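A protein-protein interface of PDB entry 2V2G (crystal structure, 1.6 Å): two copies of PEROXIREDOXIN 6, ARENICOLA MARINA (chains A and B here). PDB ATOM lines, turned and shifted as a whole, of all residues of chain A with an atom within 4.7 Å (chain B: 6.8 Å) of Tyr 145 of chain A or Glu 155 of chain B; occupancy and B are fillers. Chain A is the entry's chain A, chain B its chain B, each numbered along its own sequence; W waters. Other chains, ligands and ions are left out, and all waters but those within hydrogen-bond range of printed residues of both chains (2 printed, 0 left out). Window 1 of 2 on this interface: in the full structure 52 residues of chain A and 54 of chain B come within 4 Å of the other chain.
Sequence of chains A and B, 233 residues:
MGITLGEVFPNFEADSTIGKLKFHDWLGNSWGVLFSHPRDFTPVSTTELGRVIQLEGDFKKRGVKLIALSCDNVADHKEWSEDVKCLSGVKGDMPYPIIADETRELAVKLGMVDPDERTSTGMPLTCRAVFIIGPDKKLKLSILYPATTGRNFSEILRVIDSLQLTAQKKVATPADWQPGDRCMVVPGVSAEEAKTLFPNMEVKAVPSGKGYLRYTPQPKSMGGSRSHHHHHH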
ATOM      1  N   CYS A 127      30.249 -19.003  13.552  1.00  0.00           N
ATOM      2  CA  CYS A 127      28.907 -19.322  14.042  1.00  0.00           C
ATOM      3  C   CYS A 127      28.984 -20.252  15.274  1.00  0.00           C
ATOM      4  O   CYS A 127      29.988 -20.228  15.998  1.00  0.00           O
ATOM      5  CB  CYS A 127      28.098 -19.900  12.878  1.00  0.00           C
ATOM      6  SG  CYS A 127      28.632 -21.543  12.318  1.00  0.00           S
ATOM      7  N   ARG A 128      27.899 -20.980  15.564  1.00  0.00           N
ATOM      8  CA  ARG A 128      27.826 -21.923  16.636  1.00  0.00           C
ATOM      9  C   ARG A 128      27.896 -23.324  16.039  1.00  0.00           C
ATOM     10  O   ARG A 128      26.879 -23.999  15.776  1.00  0.00           O
ATOM     11  CB  ARG A 128      26.535 -21.706  17.397  1.00  0.00           C
ATOM     12  CG  ARG A 128      26.434 -20.398  18.130  1.00  0.00           C
ATOM     13  CD  ARG A 128      25.202 -20.262  18.986  1.00  0.00           C
ATOM     14  NE  ARG A 128      25.034 -18.855  19.330  1.00  0.00           N
ATOM     15  CZ  ARG A 128      25.786 -18.143  20.163  1.00  0.00           C
ATOM     16  NH1 ARG A 128      26.706 -18.719  20.895  1.00  0.00           N
ATOM     17  NH2 ARG A 128      25.648 -16.831  20.205  1.00  0.00           N
ATOM     18  N   ALA A 129      29.093 -23.723  15.633  1.00  0.00           N
ATOM     19  CA  ALA A 129      29.309 -24.995  14.939  1.00  0.00           C
ATOM     20  C   ALA A 129      29.643 -26.098  15.947  1.00  0.00           C
ATOM     21  O   ALA A 129      30.222 -25.818  16.974  1.00  0.00           O
ATOM     22  CB  ALA A 129      30.456 -24.838  13.874  1.00  0.00           C
ATOM     23  N   ILE A 143      27.030 -29.880  12.896  1.00  0.00           N
ATOM     24  CA  ILE A 143      25.900 -28.920  12.876  1.00  0.00           C
ATOM     25  C   ILE A 143      26.458 -27.546  12.713  1.00  0.00           C
ATOM     26  O   ILE A 143      27.532 -27.215  13.273  1.00  0.00           O
ATOM     27  CB  ILE A 143      24.932 -29.023  14.075  1.00  0.00           C
ATOM     28  CG1 ILE A 143      25.438 -28.349  15.323  1.00  0.00           C
ATOM     29  CG2 ILE A 143      24.491 -30.505  14.413  1.00  0.00           C
ATOM     30  CD1 ILE A 143      24.584 -28.483  16.606  1.00  0.00           C
ATOM     31  N   LEU A 144      25.715 -26.695  12.024  1.00  0.00           N
ATOM     32  CA  LEU A 144      26.069 -25.285  11.883  1.00  0.00           C
ATOM     33  C   LEU A 144      24.862 -24.484  12.278  1.00  0.00           C
ATOM     34  O   LEU A 144      23.889 -24.331  11.499  1.00  0.00           O
ATOM     35  CB  LEU A 144      26.468 -24.906  10.442  1.00  0.00           C
ATOM     36  CG  LEU A 144      27.726 -25.407   9.797  1.00  0.00           C
ATOM     37  CD1 LEU A 144      27.741 -24.769   8.371  1.00  0.00           C
ATOM     38  CD2 LEU A 144      28.969 -25.042  10.644  1.00  0.00           C
ATOM     39  N   TYR A 145      24.881 -24.010  13.502  1.00  0.00           N
ATOM     40  CA  TYR A 145      23.813 -23.115  13.990  1.00  0.00           C
ATOM     41  C   TYR A 145      24.307 -21.650  13.932  1.00  0.00           C
ATOM     42  O   TYR A 145      25.497 -21.378  14.183  1.00  0.00           O
ATOM     43  CB  TYR A 145      23.455 -23.426  15.451  1.00  0.00           C
ATOM     44  CG  TYR A 145      22.601 -24.654  15.695  1.00  0.00           C
ATOM     45  CD1 TYR A 145      22.532 -25.692  14.804  1.00  0.00           C
ATOM     46  CD2 TYR A 145      21.794 -24.731  16.855  1.00  0.00           C
ATOM     47  CE1 TYR A 145      21.725 -26.799  15.049  1.00  0.00           C
ATOM     48  CE2 TYR A 145      21.004 -25.835  17.114  1.00  0.00           C
ATOM     49  CZ  TYR A 145      20.955 -26.881  16.222  1.00  0.00           C
ATOM     50  OH  TYR A 145      20.151 -28.004  16.434  1.00  0.00           O
ATOM     51  N   PRO A 146      23.405 -20.694  13.635  1.00  0.00           N
ATOM     52  CA  PRO A 146      23.833 -19.308  13.610  1.00  0.00           C
ATOM     53  C   PRO A 146      23.963 -18.649  14.994  1.00  0.00           C
ATOM     54  O   PRO A 146      23.483 -19.220  16.031  1.00  0.00           O
ATOM     55  CB  PRO A 146      22.709 -18.643  12.819  1.00  0.00           C
ATOM     56  CG  PRO A 146      21.491 -19.398  13.249  1.00  0.00           C
ATOM     57  CD  PRO A 146      21.969 -20.856  13.357  1.00  0.00           C
ATOM     58  N   ALA A 147      24.529 -17.426  15.048  1.00  0.00           N
ATOM     59  CA  ALA A 147      24.722 -16.749  16.311  1.00  0.00           C
ATOM     60  C   ALA A 147      23.424 -16.556  17.101  1.00  0.00           C
ATOM     61  O   ALA A 147      23.425 -16.497  18.303  1.00  0.00           O
ATOM     62  CB  ALA A 147      25.408 -15.403  16.056  1.00  0.00           C
ATOM     63  N   THR A 149      20.997 -18.501  17.682  1.00  0.00           N
ATOM     64  CA  THR A 149      20.286 -19.759  18.049  1.00  0.00           C
ATOM     65  C   THR A 149      21.201 -20.674  18.885  1.00  0.00           C
ATOM     66  O   THR A 149      22.014 -21.417  18.360  1.00  0.00           O
ATOM     67  CB  THR A 149      19.671 -20.459  16.814  1.00  0.00           C
ATOM     68  OG1 THR A 149      18.798 -19.522  16.167  1.00  0.00           O
ATOM     69  CG2 THR A 149      18.924 -21.789  17.199  1.00  0.00           C
ATOM     70  N   GLY A 150      21.009 -20.621  20.197  1.00  0.00           N
ATOM     71  CA  GLY A 150      21.775 -21.466  21.075  1.00  0.00           C
ATOM     72  C   GLY A 150      21.530 -22.928  20.846  1.00  0.00           C
ATOM     73  O   GLY A 150      20.469 -23.320  20.447  1.00  0.00           O
ATOM     74  N   ARG A 151      22.558 -23.770  21.062  1.00  0.00           N
ATOM     75  CA  ARG A 151      22.491 -25.170  20.810  1.00  0.00           C
ATOM     76  C   ARG A 151      21.788 -25.981  21.920  1.00  0.00           C
ATOM     77  O   ARG A 151      21.447 -25.453  22.963  1.00  0.00           O
ATOM     78  CB  ARG A 151      23.910 -25.697  20.603  1.00  0.00           C
ATOM     79  CG  ARG A 151      24.487 -25.239  19.278  1.00  0.00           C
ATOM     80  CD  ARG A 151      25.948 -25.301  19.240  1.00  0.00           C
ATOM     81  NE  ARG A 151      26.557 -24.243  20.006  1.00  0.00           N
ATOM     82  CZ  ARG A 151      27.844 -23.890  19.943  1.00  0.00           C
ATOM     83  NH1 ARG A 151      28.722 -24.514  19.131  1.00  0.00           N
ATOM     84  NH2 ARG A 151      28.225 -22.856  20.610  1.00  0.00           N
ATOM     85  N   ASN A 152      21.477 -27.234  21.575  1.00  0.00           N
ATOM     86  CA  ASN A 152      20.902 -28.251  22.467  1.00  0.00           C
ATOM     87  C   ASN A 152      21.986 -29.318  22.651  1.00  0.00           C
ATOM     88  O   ASN A 152      22.172 -30.197  21.817  1.00  0.00           O
ATOM     89  CB  ASN A 152      19.601 -28.797  21.836  1.00  0.00           C
ATOM     90  CG  ASN A 152      19.008 -29.966  22.570  1.00  0.00           C
ATOM     91  OD1 ASN A 152      19.594 -30.446  23.544  1.00  0.00           O
ATOM     92  ND2 ASN A 152      17.869 -30.438  22.114  1.00  0.00           N
ATOM     93  N   LEU B   5      26.558 -20.986   6.019  1.00  0.00           N
ATOM     94  CA  LEU B   5      25.380 -20.179   6.442  1.00  0.00           C
ATOM     95  C   LEU B   5      25.391 -18.818   5.702  1.00  0.00           C
ATOM     96  O   LEU B   5      26.423 -18.187   5.503  1.00  0.00           O
ATOM     97  CB  LEU B   5      25.383 -19.985   7.936  1.00  0.00           C
ATOM     98  CG  LEU B   5      25.307 -21.236   8.765  1.00  0.00           C
ATOM     99  CD1 LEU B   5      25.157 -20.877  10.231  1.00  0.00           C
ATOM    100  CD2 LEU B   5      24.211 -22.179   8.288  1.00  0.00           C
ATOM    101  N   ILE B 132      17.779 -25.539   6.549  1.00  0.00           N
ATOM    102  CA  ILE B 132      16.650 -24.671   6.875  1.00  0.00           C
ATOM    103  C   ILE B 132      16.924 -23.365   6.097  1.00  0.00           C
ATOM    104  O   ILE B 132      17.986 -22.695   6.294  1.00  0.00           O
ATOM    105  CB  ILE B 132      16.493 -24.417   8.377  1.00  0.00           C
ATOM    106  CG1 ILE B 132      16.489 -25.719   9.184  1.00  0.00           C
ATOM    107  CG2 ILE B 132      15.207 -23.535   8.601  1.00  0.00           C
ATOM    108  CD1 ILE B 132      16.092 -25.574  10.621  1.00  0.00           C
ATOM    109  N   LYS B 140      19.982 -20.764   6.654  1.00  0.00           N
ATOM    110  CA  LYS B 140      19.958 -20.273   8.028  1.00  0.00           C
ATOM    111  C   LYS B 140      20.564 -21.180   9.060  1.00  0.00           C
ATOM    112  O   LYS B 140      21.025 -20.673  10.064  1.00  0.00           O
ATOM    113  CB  LYS B 140      18.509 -19.959   8.464  1.00  0.00           C
ATOM    114  CG  LYS B 140      17.801 -18.935   7.571  1.00  0.00           C
ATOM    115  CD  LYS B 140      18.491 -17.605   7.377  1.00  0.00           C
ATOM    116  CE  LYS B 140      17.773 -16.689   6.390  1.00  0.00           C
ATOM    117  NZ  LYS B 140      18.510 -15.394   6.305  1.00  0.00           N
ATOM    118  N   LEU B 141      20.532 -22.486   8.802  1.00  0.00           N
ATOM    119  CA  LEU B 141      21.012 -23.487   9.728  1.00  0.00           C
ATOM    120  C   LEU B 141      21.133 -24.802   8.972  1.00  0.00           C
ATOM    121  O   LEU B 141      20.261 -25.099   8.072  1.00  0.00           O
ATOM    122  CB  LEU B 141      20.030 -23.596  10.895  1.00  0.00           C
ATOM    123  CG  LEU B 141      20.260 -24.546  12.060  1.00  0.00           C
ATOM    124  CD1 LEU B 141      19.574 -24.021  13.294  1.00  0.00           C
ATOM    125  CD2 LEU B 141      19.822 -26.041  11.774  1.00  0.00           C
ATOM    126  N   SER B 142      22.203 -25.582   9.291  1.00  0.00           N
ATOM    127  CA  SER B 142      22.275 -26.908   8.711  1.00  0.00           C
ATOM    128  C   SER B 142      22.760 -27.935   9.709  1.00  0.00           C
ATOM    129  O   SER B 142      23.410 -27.587  10.658  1.00  0.00           O
ATOM    130  CB  SER B 142      23.140 -26.899   7.464  1.00  0.00           C
ATOM    131  OG  SER B 142      24.461 -26.641   7.759  1.00  0.00           O
ATOM    132  N   ILE B 143      22.360 -29.174   9.437  1.00  0.00           N
ATOM    133  CA  ILE B 143      22.889 -30.342  10.144  1.00  0.00           C
ATOM    134  C   ILE B 143      23.294 -31.414   9.132  1.00  0.00           C
ATOM    135  O   ILE B 143      22.692 -31.551   8.076  1.00  0.00           O
ATOM    136  CB  ILE B 143      21.987 -30.908  11.217  1.00  0.00           C
ATOM    137  CG1 ILE B 143      20.874 -31.775  10.667  1.00  0.00           C
ATOM    138  CG2 ILE B 143      21.464 -29.766  12.060  1.00  0.00           C
ATOM    139  CD1 ILE B 143      19.878 -32.347  11.704  1.00  0.00           C
ATOM    140  N   TYR B 145      23.956 -35.317   9.629  1.00  0.00           N
ATOM    141  CA  TYR B 145      23.994 -36.588  10.337  1.00  0.00           C
ATOM    142  C   TYR B 145      24.277 -37.764   9.384  1.00  0.00           C
ATOM    143  O   TYR B 145      23.870 -37.706   8.215  1.00  0.00           O
ATOM    144  CB  TYR B 145      22.692 -36.885  11.054  1.00  0.00           C
ATOM    145  CG  TYR B 145      22.385 -36.122  12.320  1.00  0.00           C
ATOM    146  CD1 TYR B 145      22.916 -34.875  12.578  1.00  0.00           C
ATOM    147  CD2 TYR B 145      21.479 -36.641  13.242  1.00  0.00           C
ATOM    148  CE1 TYR B 145      22.565 -34.165  13.701  1.00  0.00           C
ATOM    149  CE2 TYR B 145      21.087 -35.940  14.343  1.00  0.00           C
ATOM    150  CZ  TYR B 145      21.664 -34.722  14.609  1.00  0.00           C
ATOM    151  OH  TYR B 145      21.301 -33.965  15.704  1.00  0.00           O
ATOM    152  N   ASN B 152      16.426 -36.012  15.172  1.00  0.00           N
ATOM    153  CA  ASN B 152      15.468 -35.525  16.169  1.00  0.00           C
ATOM    154  C   ASN B 152      14.729 -34.334  15.504  1.00  0.00           C
ATOM    155  O   ASN B 152      15.205 -33.216  15.444  1.00  0.00           O
ATOM    156  CB  ASN B 152      16.277 -35.108  17.417  1.00  0.00           C
ATOM    157  CG  ASN B 152      15.408 -34.486  18.475  1.00  0.00           C
ATOM    158  OD1 ASN B 152      14.225 -34.294  18.240  1.00  0.00           O
ATOM    159  ND2 ASN B 152      15.970 -34.208  19.608  1.00  0.00           N
ATOM    160  N   PHE B 153      13.535 -34.591  14.934  1.00  0.00           N
ATOM    161  CA  PHE B 153      12.788 -33.504  14.294  1.00  0.00           C
ATOM    162  C   PHE B 153      12.119 -32.525  15.285  1.00  0.00           C
ATOM    163  O   PHE B 153      11.822 -31.433  14.854  1.00  0.00           O
ATOM    164  CB  PHE B 153      11.749 -34.039  13.289  1.00  0.00           C
ATOM    165  CG  PHE B 153      12.387 -34.692  12.128  1.00  0.00           C
ATOM    166  CD1 PHE B 153      12.713 -36.045  12.214  1.00  0.00           C
ATOM    167  CD2 PHE B 153      12.819 -33.972  11.025  1.00  0.00           C
ATOM    168  CE1 PHE B 153      13.373 -36.682  11.161  1.00  0.00           C
ATOM    169  CE2 PHE B 153      13.479 -34.639   9.940  1.00  0.00           C
ATOM    170  CZ  PHE B 153      13.768 -35.986  10.071  1.00  0.00           C
ATOM    171  N   SER B 154      11.994 -32.899  16.527  1.00  0.00           N
ATOM    172  CA  SER B 154      11.630 -31.941  17.586  1.00  0.00           C
ATOM    173  C   SER B 154      12.675 -30.832  17.717  1.00  0.00           C
ATOM    174  O   SER B 154      12.341 -29.660  17.907  1.00  0.00           O
ATOM    175  CB  SER B 154      11.408 -32.574  18.927  1.00  0.00           C
ATOM    176  OG  SER B 154      10.286 -33.413  18.802  1.00  0.00           O
ATOM    177  N   GLU B 155      13.943 -31.224  17.595  1.00  0.00           N
ATOM    178  CA  GLU B 155      15.022 -30.223  17.636  1.00  0.00           C
ATOM    179  C   GLU B 155      14.909 -29.277  16.434  1.00  0.00           C
ATOM    180  O   GLU B 155      15.202 -28.088  16.531  1.00  0.00           O
ATOM    181  CB  GLU B 155      16.412 -30.888  17.625  1.00  0.00           C
ATOM    182  CG  GLU B 155      17.622 -29.864  17.522  1.00  0.00           C
ATOM    183  CD  GLU B 155      17.701 -28.857  18.615  1.00  0.00           C
ATOM    184  OE1 GLU B 155      16.951 -28.990  19.636  1.00  0.00           O
ATOM    185  OE2 GLU B 155      18.551 -27.937  18.506  1.00  0.00           O
ATOM    186  N   ILE B 156      14.540 -29.829  15.276  1.00  0.00           N
ATOM    187  CA  ILE B 156      14.351 -29.023  14.096  1.00  0.00           C
ATOM    188  C   ILE B 156      13.221 -28.008  14.291  1.00  0.00           C
ATOM    189  O   ILE B 156      13.378 -26.829  13.938  1.00  0.00           O
ATOM    190  CB  ILE B 156      14.097 -29.884  12.831  1.00  0.00           C
ATOM    191  CG1 ILE B 156      15.344 -30.753  12.595  1.00  0.00           C
ATOM    192  CG2 ILE B 156      13.788 -29.009  11.607  1.00  0.00           C
ATOM    193  CD1 ILE B 156      15.229 -31.837  11.599  1.00  0.00           C
ATOM    194  N   LEU B 157      12.133 -28.443  14.914  1.00  0.00           N
ATOM    195  CA  LEU B 157      11.032 -27.517  15.263  1.00  0.00           C
ATOM    196  C   LEU B 157      11.528 -26.459  16.244  1.00  0.00           C
ATOM    197  O   LEU B 157      11.237 -25.253  16.083  1.00  0.00           O
ATOM    198  CB  LEU B 157       9.782 -28.237  15.767  1.00  0.00           C
ATOM    199  CG  LEU B 157       9.051 -29.002  14.669  1.00  0.00           C
ATOM    200  CD1 LEU B 157       8.008 -29.961  15.235  1.00  0.00           C
ATOM    201  CD2 LEU B 157       8.352 -28.046  13.668  1.00  0.00           C
ATOM    202  N   ARG B 158      12.331 -26.909  17.218  1.00  0.00           N
ATOM    203  CA  ARG B 158      12.829 -25.942  18.241  1.00  0.00           C
ATOM    204  C   ARG B 158      13.637 -24.831  17.566  1.00  0.00           C
ATOM    205  O   ARG B 158      13.433 -23.618  17.844  1.00  0.00           O
ATOM    206  CB  ARG B 158      13.641 -26.676  19.332  1.00  0.00           C
ATOM    207  CG  ARG B 158      14.065 -25.765  20.523  1.00  0.00           C
ATOM    208  CD  ARG B 158      15.032 -26.454  21.456  1.00  0.00           C
ATOM    209  NE  ARG B 158      16.350 -26.500  20.824  1.00  0.00           N
ATOM    210  CZ  ARG B 158      17.224 -25.512  20.896  1.00  0.00           C
ATOM    211  NH1 ARG B 158      16.940 -24.400  21.582  1.00  0.00           N
ATOM    212  NH2 ARG B 158      18.358 -25.601  20.229  1.00  0.00           N
ATOM    213  N   VAL B 159      14.613 -25.209  16.732  1.00  0.00           N
ATOM    214  CA  VAL B 159      15.444 -24.212  16.079  1.00  0.00           C
ATOM    215  C   VAL B 159      14.642 -23.303  15.068  1.00  0.00           C
ATOM    216  O   VAL B 159      14.969 -22.116  14.945  1.00  0.00           O
ATOM    217  CB  VAL B 159      16.720 -24.828  15.469  1.00  0.00           C
ATOM    218  CG1 VAL B 159      17.591 -25.435  16.608  1.00  0.00           C
ATOM    219  CG2 VAL B 159      16.419 -25.872  14.337  1.00  0.00           C
ATOM    220  N   ILE B 160      13.629 -23.855  14.373  1.00  0.00           N
ATOM    221  CA  ILE B 160      12.678 -23.030  13.550  1.00  0.00           C
ATOM    222  C   ILE B 160      12.052 -21.948  14.379  1.00  0.00           C
ATOM    223  O   ILE B 160      12.010 -20.802  13.984  1.00  0.00           O
ATOM    224  CB  ILE B 160      11.669 -23.886  12.829  1.00  0.00           C
ATOM    225  CG1 ILE B 160      12.351 -24.738  11.733  1.00  0.00           C
ATOM    226  CG2 ILE B 160      10.489 -22.992  12.283  1.00  0.00           C
ATOM    227  CD1 ILE B 160      11.395 -25.894  11.202  1.00  0.00           C
ATOM    228  N   TRP B 177      17.034 -23.453  25.126  1.00  0.00           N
ATOM    229  CA  TRP B 177      15.783 -22.658  25.058  1.00  0.00           C
ATOM    230  C   TRP B 177      14.626 -23.430  24.432  1.00  0.00           C
ATOM    231  O   TRP B 177      14.793 -24.086  23.398  1.00  0.00           O
ATOM    232  CB  TRP B 177      16.013 -21.374  24.285  1.00  0.00           C
ATOM    233  CG  TRP B 177      14.789 -20.558  24.013  1.00  0.00           C
ATOM    234  CD1 TRP B 177      14.277 -19.558  24.761  1.00  0.00           C
ATOM    235  CD2 TRP B 177      14.012 -20.611  22.793  1.00  0.00           C
ATOM    236  NE1 TRP B 177      13.201 -18.982  24.097  1.00  0.00           N
ATOM    237  CE2 TRP B 177      13.011 -19.617  22.895  1.00  0.00           C
ATOM    238  CE3 TRP B 177      14.052 -21.422  21.640  1.00  0.00           C
ATOM    239  CZ2 TRP B 177      12.043 -19.431  21.890  1.00  0.00           C
ATOM    240  CZ3 TRP B 177      13.154 -21.190  20.664  1.00  0.00           C
ATOM    241  CH2 TRP B 177      12.132 -20.235  20.809  1.00  0.00           C
ATOM    242  N   GLN B 178      13.436 -23.328  25.052  1.00  0.00           N
ATOM    243  CA  GLN B 178      12.164 -23.819  24.495  1.00  0.00           C
ATOM    244  C   GLN B 178      11.280 -22.569  24.371  1.00  0.00           C
ATOM    245  O   GLN B 178      11.424 -21.655  25.212  1.00  0.00           O
ATOM    246  CB  GLN B 178      11.518 -24.828  25.396  1.00  0.00           C
ATOM    247  CG  GLN B 178      12.270 -26.166  25.482  1.00  0.00           C
ATOM    248  CD  GLN B 178      12.195 -26.983  24.179  1.00  0.00           C
ATOM    249  OE1 GLN B 178      13.112 -27.727  23.839  1.00  0.00           O
ATOM    250  NE2 GLN B 178      11.090 -26.841  23.446  1.00  0.00           N
HETATM  251  O   HOH W   1      14.575 -30.357  21.097  1.00  0.00           O
HETATM  252  O   HOH W   2      18.453 -21.872  21.588  1.00  0.00           O
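SG of Cys 127 of chain A lies close to O of Tyr 145 of chain A (3.7 Å).
O of Trp 177 of chain B is in hydrogen-bond range of NH1 of Arg 158 of chain B.
The backbone carbonyl oxygen (O) of Ala 129 of chain A sits at hydrogen-bond distance from the guanidinium group (NH1) of Arg 151 of chain A, 2.9 Å away.
The backbone NH (N) of Arg 128 of chain A lies within hydrogen-bond range of the backbone carbonyl oxygen (O) of Tyr 145 of chain A, 2.8 Å away.
The side-chain amide oxygen (OD1) of Asn 152 of chain B is in hydrogen-bond range of the backbone NH (N) of Glu 155 of chain B.
N of Lys 140 of chain B lies within hydrogen-bond range of O of Ile 132 of chain B (2.8 Å).
Of the 18 printed residues of chain B, 8 touch a printed residue of chain A.
Hydrophobic or aromatic side chains of chain B that line the printed part of chain A: Leu 5, Leu 141, Ile 143 and Val 159.
CA of Ile 143 of chain A touches O of Ser 142 of chain B (3.6 Å).
Ile 143 of chain A touches Ile 143 of chain B.
Leu 144 of chain A touches Leu 141 of chain B.
Leu 5 of chain B touches Tyr 145 of chain A (CD1 to C, 3.9 Å).
Tyr 145 of chain A touches Leu 141 of chain B (CD1 to CD1, 3.7 Å).
CG1 of Val 159 of chain B touches CE2 of Tyr 145 of chain A, 3.5 Å away.
Pro 146 of chain A touches Leu 5 of chain B.
CD1 of Leu 141 of chain B touches CD of Pro 146 of chain A, at 3.97 Å.
CG2 of Thr 149 of chain A touches CG1 of Val 159 of chain B, at 3.9 Å.
N of Asn 152 of chain A touches NH2 of Arg 158 of chain B (3.8 Å).
Water W2 bridges the backbone carbonyl oxygen (O) of Gly 150 of chain A (2.7 Å) and the guanidinium group (NH1) of Arg 158 of chain B (2.9 Å).
Water W1 bridges the side-chain carboxylate (OE1) of Glu 155 of chain B (3.1 Å) and the side-chain amide nitrogen (ND2) of Asn 152 of chain A (3.4 Å).
Of chain B, only Leu 5 (3.9 Å), Leu 141 (3.7 Å), Glu 155 (2.6 Å) and Val 159 (3.5 Å) come within 4 Å of Tyr 145 of chain A.
Of chain A, only Tyr 145 and Asn 152 come within 4 Å of Glu 155 of chain B.
Of the printed residues of chain B, Pro 146 of chain A touches Leu 5 (3.8 Å), Lys 140 (3.4 Å) and Leu 141 (3.97 Å).
Of the printed residues of chain B, Ile 143 of chain A touches Ser 142 and Ile 143.
Printed residues of chain A within 4 Å of Arg 158 of chain B: Gly 150 (3.1 Å), Arg 151 (3.8 Å) and Asn 152 (3.8 Å).
Of the printed residues of chain A, Lys 140 of chain B touches Pro 146.
Ile 156 of chain B touches none of the printed residues of chain A.
Phe 153 of chain B touches none of the printed residues of chain A.
The nearest printed residue of chain A that does not touch Glu 155 of chain B is Arg 151 of chain A (5.1 Å).
The nearest printed residue of chain A that does not touch Ser 142 of chain B is Tyr 145 of chain A (4.6 Å).
Ile 143 of chain A touches its own counterpart, Ile 143 of chain B.
3 positions are printed for both chains.
Of the 17 pairs that touch across the chains among the printed residues, 1 has its exchanged pair printed and touching as well.
The backbone carbonyl oxygen of Ser 142 of chain B is in hydrogen-bond range of the backbone NH of Leu 144 of chain A (2.8 Å).
ND2 of Asn 152 of chain A sits at hydrogen-bond distance from OE1 of Glu 155 of chain B, at 3.0 Å.
The side-chain carboxylate (OE2) of Glu 155 of chain B is in hydrogen-bond range of the side-chain hydroxyl (OH) of Tyr 145 of chain A, 2.6 Å away.
The guanidinium group (NH2) of Arg 158 of chain B lies within hydrogen-bond range of the backbone carbonyl oxygen (O) of Gly 150 of chain A, 3.1 Å away.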
